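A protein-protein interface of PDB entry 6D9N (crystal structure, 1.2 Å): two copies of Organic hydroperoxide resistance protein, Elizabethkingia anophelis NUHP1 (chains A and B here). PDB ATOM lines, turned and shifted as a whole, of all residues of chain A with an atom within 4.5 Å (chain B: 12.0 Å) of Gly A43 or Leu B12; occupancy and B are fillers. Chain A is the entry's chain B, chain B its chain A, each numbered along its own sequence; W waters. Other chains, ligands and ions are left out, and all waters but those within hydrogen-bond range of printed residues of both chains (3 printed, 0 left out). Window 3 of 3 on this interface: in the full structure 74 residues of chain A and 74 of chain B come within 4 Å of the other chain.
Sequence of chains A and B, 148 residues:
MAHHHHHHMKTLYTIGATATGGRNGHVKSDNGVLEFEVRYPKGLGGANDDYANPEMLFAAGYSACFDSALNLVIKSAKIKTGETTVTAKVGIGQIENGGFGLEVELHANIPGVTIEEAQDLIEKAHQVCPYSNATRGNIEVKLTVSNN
The side-chain sulfur (SD) of Met B9 is in hydrogen-bond range of the backbone NH (N) of Gly A93, 3.5 Å away. N of Leu B12 lies within hydrogen-bond range of O of Ile A92 (2.8 Å). N of Ile A92 lies within hydrogen-bond range of O of Tyr B13 (3.0 Å). The backbone carbonyl oxygen (O) of Val B128 sits at hydrogen-bond distance from the backbone NH (N) of Phe A100, 3.1 Å away.
Water W3 bridges the backbone carbonyl oxygen of Gln A94 (2.5 Å) and the backbone NH of Lys B10 (2.8 Å). Water W2 lies within hydrogen-bond range of the backbone carbonyl oxygen (O) of Lys B10 (2.5 Å) and the backbone NH (N) of Gln A94 (2.9 Å). Water W1 lies within hydrogen-bond range of O of Gly A43 (2.6 Å) and O of Leu B12 (2.8 Å).
Printed residues of chain B within 4 Å of Gly A43: Leu B12. Leu B12 touches three residues of chain A. Printed residues of chain B within 4 Å of Pro A41: Tyr B13. No residue of chain B comes within 4 Å of Lys A42. Leu A44 touches two residues of chain B. Gly A45 touches none of the printed residues of chain B. Ile A92 touches just these residues of chain B: Met B9, Thr B11, Leu B12, Tyr B13 and Pro B130. Gln A94 touches just one residue of chain B: Met B9. Of the printed residues of chain A, Lys B10 touches Gly A93 (3.6 Å). Of the printed residues of chain B, Phe A100 touches Val B128 and Pro B130. Of the printed residues of chain A, Met B9 touches Ile A92, Gly A93 and Gln A94. Printed residues of chain A within 4 Å of Thr B11: Ile A92. Of the printed residues of chain A, Tyr B13 touches Pro A41, Leu A44 and Ile A92. Leu B72 touches none of the printed residues of chain A. The nearest residue of chain B that does not touch Gly A43 is Tyr B13 (4.6 Å). The nearest residue of chain A that does not touch Leu B12 is Gly A93 (4.2 Å). The nearest printed residue of chain A that does not touch Lys B10 is Gln A94 (4.3 Å).
Among the printed residues, merely in contact across the chains: Phe A100 with Pro B130 (3.3 Å), Pro A41 with Tyr B13 (3.5 Å), Leu A44 with Leu B12 (3.6 Å), Gly A93 with Lys B10 (3.6 Å), Gln A94 with Met B9 (3.7 Å), Ile A92 with Thr B11 (3.7 Å), Ile A92 with Pro B130 (3.7 Å), Gly A43 with Leu B12 (3.7 Å), Leu A44 with Tyr B13 (3.8 Å) and Ile A92 with Met B9 (3.9 Å).
No position is printed for both chains. Of the 14 pairs that touch across the chains among the printed residues, none has its exchanged pair printed and touching as well.
Hydrophobic or aromatic side chains of chain A that line the printed part of chain B: Pro A41, Leu A44, Ile A92 and Phe A100. Of the 13 printed residues of chain B, 7 touch a printed residue of chain A. Hydrophobic or aromatic side chains of chain B within 4 Å of the printed part of chain A: Met B9, Leu B12, Tyr B13 and Pro B130. Among the printed residues, no Asp or Glu carboxylate lies within 4 Å of a Lys or Arg side-chain nitrogen of the other chain.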
ATOM      1  N   PRO A  41     -23.718  -2.645 -23.540  1.00  0.00           N
ATOM      2  CA  PRO A  41     -22.667  -3.139 -24.425  1.00  0.00           C
ATOM      3  C   PRO A  41     -22.046  -1.973 -25.183  1.00  0.00           C
ATOM      4  O   PRO A  41     -22.590  -0.875 -25.232  1.00  0.00           O
ATOM      5  CB  PRO A  41     -23.429  -4.069 -25.370  1.00  0.00           C
ATOM      6  CG  PRO A  41     -24.776  -3.434 -25.468  1.00  0.00           C
ATOM      7  CD  PRO A  41     -25.064  -2.984 -24.055  1.00  0.00           C
ATOM      8  N   LYS A  42     -20.892  -2.241 -25.792  1.00  0.00           N
ATOM      9  CA  LYS A  42     -20.162  -1.196 -26.496  1.00  0.00           C
ATOM     10  C   LYS A  42     -21.023  -0.551 -27.575  1.00  0.00           C
ATOM     11  O   LYS A  42     -21.013   0.681 -27.738  1.00  0.00           O
ATOM     12  CB  LYS A  42     -18.891  -1.803 -27.080  1.00  0.00           C
ATOM     13  CG  LYS A  42     -17.878  -0.834 -27.601  1.00  0.00           C
ATOM     14  CD  LYS A  42     -16.466  -1.424 -27.471  1.00  0.00           C
ATOM     15  CE  LYS A  42     -16.369  -2.794 -28.123  1.00  0.00           C
ATOM     16  NZ  LYS A  42     -15.571  -2.793 -29.406  1.00  0.00           N
ATOM     17  N   GLY A  43     -21.833  -1.363 -28.274  1.00  0.00           N
ATOM     18  CA  GLY A  43     -22.596  -0.794 -29.358  1.00  0.00           C
ATOM     19  C   GLY A  43     -23.692   0.141 -28.909  1.00  0.00           C
ATOM     20  O   GLY A  43     -24.237   0.879 -29.748  1.00  0.00           O
ATOM     21  N   LEU A  44     -24.034   0.131 -27.613  1.00  0.00           N
ATOM     22  CA  LEU A  44     -25.005   1.069 -27.054  1.00  0.00           C
ATOM     23  C   LEU A  44     -24.339   2.178 -26.245  1.00  0.00           C
ATOM     24  O   LEU A  44     -25.037   2.876 -25.497  1.00  0.00           O
ATOM     25  CB  LEU A  44     -26.073   0.346 -26.221  1.00  0.00           C
ATOM     26  CG  LEU A  44     -26.944  -0.649 -27.005  1.00  0.00           C
ATOM     27  CD1 LEU A  44     -27.986  -1.348 -26.138  1.00  0.00           C
ATOM     28  CD2 LEU A  44     -27.621   0.045 -28.198  1.00  0.00           C
ATOM     29  N   GLY A  45     -23.017   2.355 -26.379  1.00  0.00           N
ATOM     30  CA  GLY A  45     -22.280   3.390 -25.670  1.00  0.00           C
ATOM     31  C   GLY A  45     -21.583   2.913 -24.425  1.00  0.00           C
ATOM     32  O   GLY A  45     -21.024   3.756 -23.684  1.00  0.00           O
ATOM     33  N   ILE A  92     -31.983  -4.449 -31.024  1.00  0.00           N
ATOM     34  CA  ILE A  92     -32.665  -3.348 -30.355  1.00  0.00           C
ATOM     35  C   ILE A  92     -32.453  -2.083 -31.170  1.00  0.00           C
ATOM     36  O   ILE A  92     -31.363  -1.850 -31.704  1.00  0.00           O
ATOM     37  CB  ILE A  92     -32.180  -3.168 -28.889  1.00  0.00           C
ATOM     38  CG1 ILE A  92     -32.923  -2.016 -28.187  1.00  0.00           C
ATOM     39  CG2 ILE A  92     -30.656  -2.967 -28.791  1.00  0.00           C
ATOM     40  CD1 ILE A  92     -32.576  -1.719 -26.758  1.00  0.00           C
ATOM     41  N   GLY A  93     -33.498  -1.262 -31.245  1.00  0.00           N
ATOM     42  CA  GLY A  93     -33.361   0.039 -31.873  1.00  0.00           C
ATOM     43  C   GLY A  93     -34.420   0.979 -31.357  1.00  0.00           C
ATOM     44  O   GLY A  93     -35.249   0.616 -30.527  1.00  0.00           O
ATOM     45  N   GLN A  94     -34.333   2.245 -31.780  1.00  0.00           N
ATOM     46  CA  GLN A  94     -35.292   3.236 -31.323  1.00  0.00           C
ATOM     47  C   GLN A  94     -36.578   3.121 -32.133  1.00  0.00           C
ATOM     48  O   GLN A  94     -36.538   2.968 -33.360  1.00  0.00           O
ATOM     49  CB  GLN A  94     -34.694   4.652 -31.441  1.00  0.00           C
ATOM     50  CG  GLN A  94     -35.483   5.740 -30.649  1.00  0.00           C
ATOM     51  CD  GLN A  94     -34.592   6.834 -30.029  1.00  0.00           C
ATOM     52  OE1 GLN A  94     -33.641   7.313 -30.662  1.00  0.00           O
ATOM     53  NE2 GLN A  94     -34.918   7.247 -28.793  1.00  0.00           N
ATOM     54  N   PHE A 100     -37.605   2.230 -27.010  1.00  0.00           N
ATOM     55  CA  PHE A 100     -36.811   1.243 -27.735  1.00  0.00           C
ATOM     56  C   PHE A 100     -37.602  -0.044 -27.930  1.00  0.00           C
ATOM     57  O   PHE A 100     -38.474  -0.396 -27.126  1.00  0.00           O
ATOM     58  CB  PHE A 100     -35.487   0.951 -27.006  1.00  0.00           C
ATOM     59  CG  PHE A 100     -34.613   2.161 -26.884  1.00  0.00           C
ATOM     60  CD1 PHE A 100     -34.730   3.041 -25.792  1.00  0.00           C
ATOM     61  CD2 PHE A 100     -33.727   2.496 -27.890  1.00  0.00           C
ATOM     62  CE1 PHE A 100     -33.941   4.199 -25.698  1.00  0.00           C
ATOM     63  CE2 PHE A 100     -32.920   3.642 -27.784  1.00  0.00           C
ATOM     64  CZ  PHE A 100     -33.042   4.479 -26.699  1.00  0.00           C
ATOM     65  N   MET B   9     -36.899  -0.090 -38.447  1.00  0.00           N
ATOM     66  CA  MET B   9     -36.124   0.277 -37.266  1.00  0.00           C
ATOM     67  C   MET B   9     -34.629   0.273 -37.587  1.00  0.00           C
ATOM     68  O   MET B   9     -34.138  -0.649 -38.240  1.00  0.00           O
ATOM     69  CB  MET B   9     -36.417  -0.715 -36.137  1.00  0.00           C
ATOM     70  CG  MET B   9     -35.848  -0.343 -34.807  1.00  0.00           C
ATOM     71  SD  MET B   9     -36.198  -1.501 -33.447  1.00  0.00           S
ATOM     72  CE  MET B   9     -35.163  -2.898 -33.874  1.00  0.00           C
ATOM     73  N   LYS B  10     -33.905   1.287 -37.115  1.00  0.00           N
ATOM     74  CA  LYS B  10     -32.452   1.363 -37.272  1.00  0.00           C
ATOM     75  C   LYS B  10     -31.823   0.573 -36.124  1.00  0.00           C
ATOM     76  O   LYS B  10     -31.780   1.039 -34.985  1.00  0.00           O
ATOM     77  CB  LYS B  10     -32.025   2.822 -37.267  1.00  0.00           C
ATOM     78  CG  LYS B  10     -30.552   3.107 -37.401  1.00  0.00           C
ATOM     79  CD  LYS B  10     -30.440   4.632 -37.425  1.00  0.00           C
ATOM     80  CE  LYS B  10     -29.047   5.173 -37.657  1.00  0.00           C
ATOM     81  NZ  LYS B  10     -29.113   6.675 -37.586  1.00  0.00           N
ATOM     82  N   THR B  11     -31.335  -0.630 -36.406  1.00  0.00           N
ATOM     83  CA  THR B  11     -30.865  -1.502 -35.339  1.00  0.00           C
ATOM     84  C   THR B  11     -29.539  -0.986 -34.784  1.00  0.00           C
ATOM     85  O   THR B  11     -28.592  -0.744 -35.549  1.00  0.00           O
ATOM     86  CB  THR B  11     -30.741  -2.908 -35.894  1.00  0.00           C
ATOM     87  OG1 THR B  11     -32.028  -3.261 -36.413  1.00  0.00           O
ATOM     88  CG2 THR B  11     -30.334  -3.841 -34.801  1.00  0.00           C
ATOM     89  N   LEU B  12     -29.480  -0.798 -33.459  1.00  0.00           N
ATOM     90  CA  LEU B  12     -28.281  -0.260 -32.831  1.00  0.00           C
ATOM     91  C   LEU B  12     -27.337  -1.347 -32.339  1.00  0.00           C
ATOM     92  O   LEU B  12     -26.111  -1.136 -32.295  1.00  0.00           O
ATOM     93  CB  LEU B  12     -28.702   0.560 -31.617  1.00  0.00           C
ATOM     94  CG  LEU B  12     -29.544   1.790 -31.975  1.00  0.00           C
ATOM     95  CD1 LEU B  12     -30.079   2.471 -30.708  1.00  0.00           C
ATOM     96  CD2 LEU B  12     -28.783   2.788 -32.852  1.00  0.00           C
ATOM     97  N   TYR B  13     -27.880  -2.501 -31.954  1.00  0.00           N
ATOM     98  CA  TYR B  13     -27.098  -3.568 -31.342  1.00  0.00           C
ATOM     99  C   TYR B  13     -27.844  -4.871 -31.563  1.00  0.00           C
ATOM    100  O   TYR B  13     -29.075  -4.903 -31.453  1.00  0.00           O
ATOM    101  CB  TYR B  13     -26.951  -3.288 -29.832  1.00  0.00           C
ATOM    102  CG  TYR B  13     -26.361  -4.411 -29.002  1.00  0.00           C
ATOM    103  CD1 TYR B  13     -25.006  -4.681 -29.017  1.00  0.00           C
ATOM    104  CD2 TYR B  13     -27.186  -5.209 -28.214  1.00  0.00           C
ATOM    105  CE1 TYR B  13     -24.453  -5.693 -28.241  1.00  0.00           C
ATOM    106  CE2 TYR B  13     -26.672  -6.233 -27.437  1.00  0.00           C
ATOM    107  CZ  TYR B  13     -25.307  -6.486 -27.448  1.00  0.00           C
ATOM    108  OH  TYR B  13     -24.790  -7.490 -26.643  1.00  0.00           O
ATOM    109  N   THR B  14     -27.097  -5.938 -31.840  1.00  0.00           N
ATOM    110  CA  THR B  14     -27.674  -7.277 -31.973  1.00  0.00           C
ATOM    111  C   THR B  14     -26.828  -8.261 -31.186  1.00  0.00           C
ATOM    112  O   THR B  14     -25.600  -8.132 -31.116  1.00  0.00           O
ATOM    113  CB  THR B  14     -27.778  -7.716 -33.478  1.00  0.00           C
ATOM    114  OG1 THR B  14     -28.608  -6.791 -34.200  1.00  0.00           O
ATOM    115  CG2 THR B  14     -28.387  -9.102 -33.634  1.00  0.00           C
ATOM    116  N   ILE B  15     -27.488  -9.273 -30.597  1.00  0.00           N
ATOM    117  CA  ILE B  15     -26.799 -10.314 -29.831  1.00  0.00           C
ATOM    118  C   ILE B  15     -27.546 -11.625 -30.055  1.00  0.00           C
ATOM    119  O   ILE B  15     -28.783 -11.644 -30.078  1.00  0.00           O
ATOM    120  CB  ILE B  15     -26.725  -9.939 -28.332  1.00  0.00           C
ATOM    121  CG1 ILE B  15     -25.891 -10.928 -27.493  1.00  0.00           C
ATOM    122  CG2 ILE B  15     -28.119  -9.671 -27.764  1.00  0.00           C
ATOM    123  CD1 ILE B  15     -24.467 -11.151 -27.922  1.00  0.00           C
ATOM    124  N   GLY B  16     -26.795 -12.726 -30.182  1.00  0.00           N
ATOM    125  CA  GLY B  16     -27.394 -14.031 -30.375  1.00  0.00           C
ATOM    126  C   GLY B  16     -27.138 -14.983 -29.226  1.00  0.00           C
ATOM    127  O   GLY B  16     -26.204 -14.825 -28.436  1.00  0.00           O
ATOM    128  N   ASN B  31     -21.041 -14.813 -27.769  1.00  0.00           N
ATOM    129  CA  ASN B  31     -19.734 -14.369 -27.318  1.00  0.00           C
ATOM    130  C   ASN B  31     -19.265 -15.107 -26.071  1.00  0.00           C
ATOM    131  O   ASN B  31     -18.191 -14.781 -25.540  1.00  0.00           O
ATOM    132  CB  ASN B  31     -19.728 -12.834 -27.128  1.00  0.00           C
ATOM    133  CG  ASN B  31     -20.755 -12.337 -26.140  1.00  0.00           C
ATOM    134  OD1 ASN B  31     -21.454 -13.111 -25.462  1.00  0.00           O
ATOM    135  ND2 ASN B  31     -20.851 -11.002 -26.068  1.00  0.00           N
ATOM    136  N   SER B  68     -33.175  -0.432 -16.190  1.00  0.00           N
ATOM    137  CA  SER B  68     -32.345   0.374 -17.097  1.00  0.00           C
ATOM    138  C   SER B  68     -33.151   1.533 -17.673  1.00  0.00           C
ATOM    139  O   SER B  68     -32.697   2.690 -17.681  1.00  0.00           O
ATOM    140  CB  SER B  68     -31.849  -0.522 -18.252  1.00  0.00           C
ATOM    141  OG  SER B  68     -31.252   0.242 -19.284  1.00  0.00           O
ATOM    142  N   LEU B  72     -32.631   5.627 -17.175  1.00  0.00           N
ATOM    143  CA  LEU B  72     -32.480   6.587 -18.269  1.00  0.00           C
ATOM    144  C   LEU B  72     -33.479   7.728 -18.139  1.00  0.00           C
ATOM    145  O   LEU B  72     -33.127   8.903 -18.361  1.00  0.00           O
ATOM    146  CB  LEU B  72     -32.621   5.903 -19.629  1.00  0.00           C
ATOM    147  CG  LEU B  72     -31.480   4.969 -20.006  1.00  0.00           C
ATOM    148  CD1 LEU B  72     -31.732   4.349 -21.380  1.00  0.00           C
ATOM    149  CD2 LEU B  72     -30.121   5.679 -19.951  1.00  0.00           C
ATOM    150  N   VAL B 128     -40.415   3.070 -22.535  1.00  0.00           N
ATOM    151  CA  VAL B 128     -39.031   3.030 -23.012  1.00  0.00           C
ATOM    152  C   VAL B 128     -38.526   1.593 -23.136  1.00  0.00           C
ATOM    153  O   VAL B 128     -37.897   1.236 -24.136  1.00  0.00           O
ATOM    154  CB  VAL B 128     -38.159   3.872 -22.060  1.00  0.00           C
ATOM    155  CG1 VAL B 128     -36.703   3.704 -22.373  1.00  0.00           C
ATOM    156  CG2 VAL B 128     -38.539   5.363 -22.164  1.00  0.00           C
ATOM    157  N   PRO B 130     -37.781  -2.057 -23.905  1.00  0.00           N
ATOM    158  CA  PRO B 130     -38.187  -2.921 -25.019  1.00  0.00           C
ATOM    159  C   PRO B 130     -39.048  -4.095 -24.612  1.00  0.00           C
ATOM    160  O   PRO B 130     -39.899  -4.529 -25.402  1.00  0.00           O
ATOM    161  CB  PRO B 130     -36.853  -3.372 -25.647  1.00  0.00           C
ATOM    162  CG  PRO B 130     -35.981  -2.244 -25.430  1.00  0.00           C
ATOM    163  CD  PRO B 130     -36.376  -1.639 -24.054  1.00  0.00           C
HETATM  164  O   HOH W   1     -24.444   1.055 -32.362  1.00  0.00           O
HETATM  165  O   HOH W   2     -32.462   3.165 -33.775  1.00  0.00           O
HETATM  166  O   HOH W   3     -35.078   3.153 -35.371  1.00  0.00           O
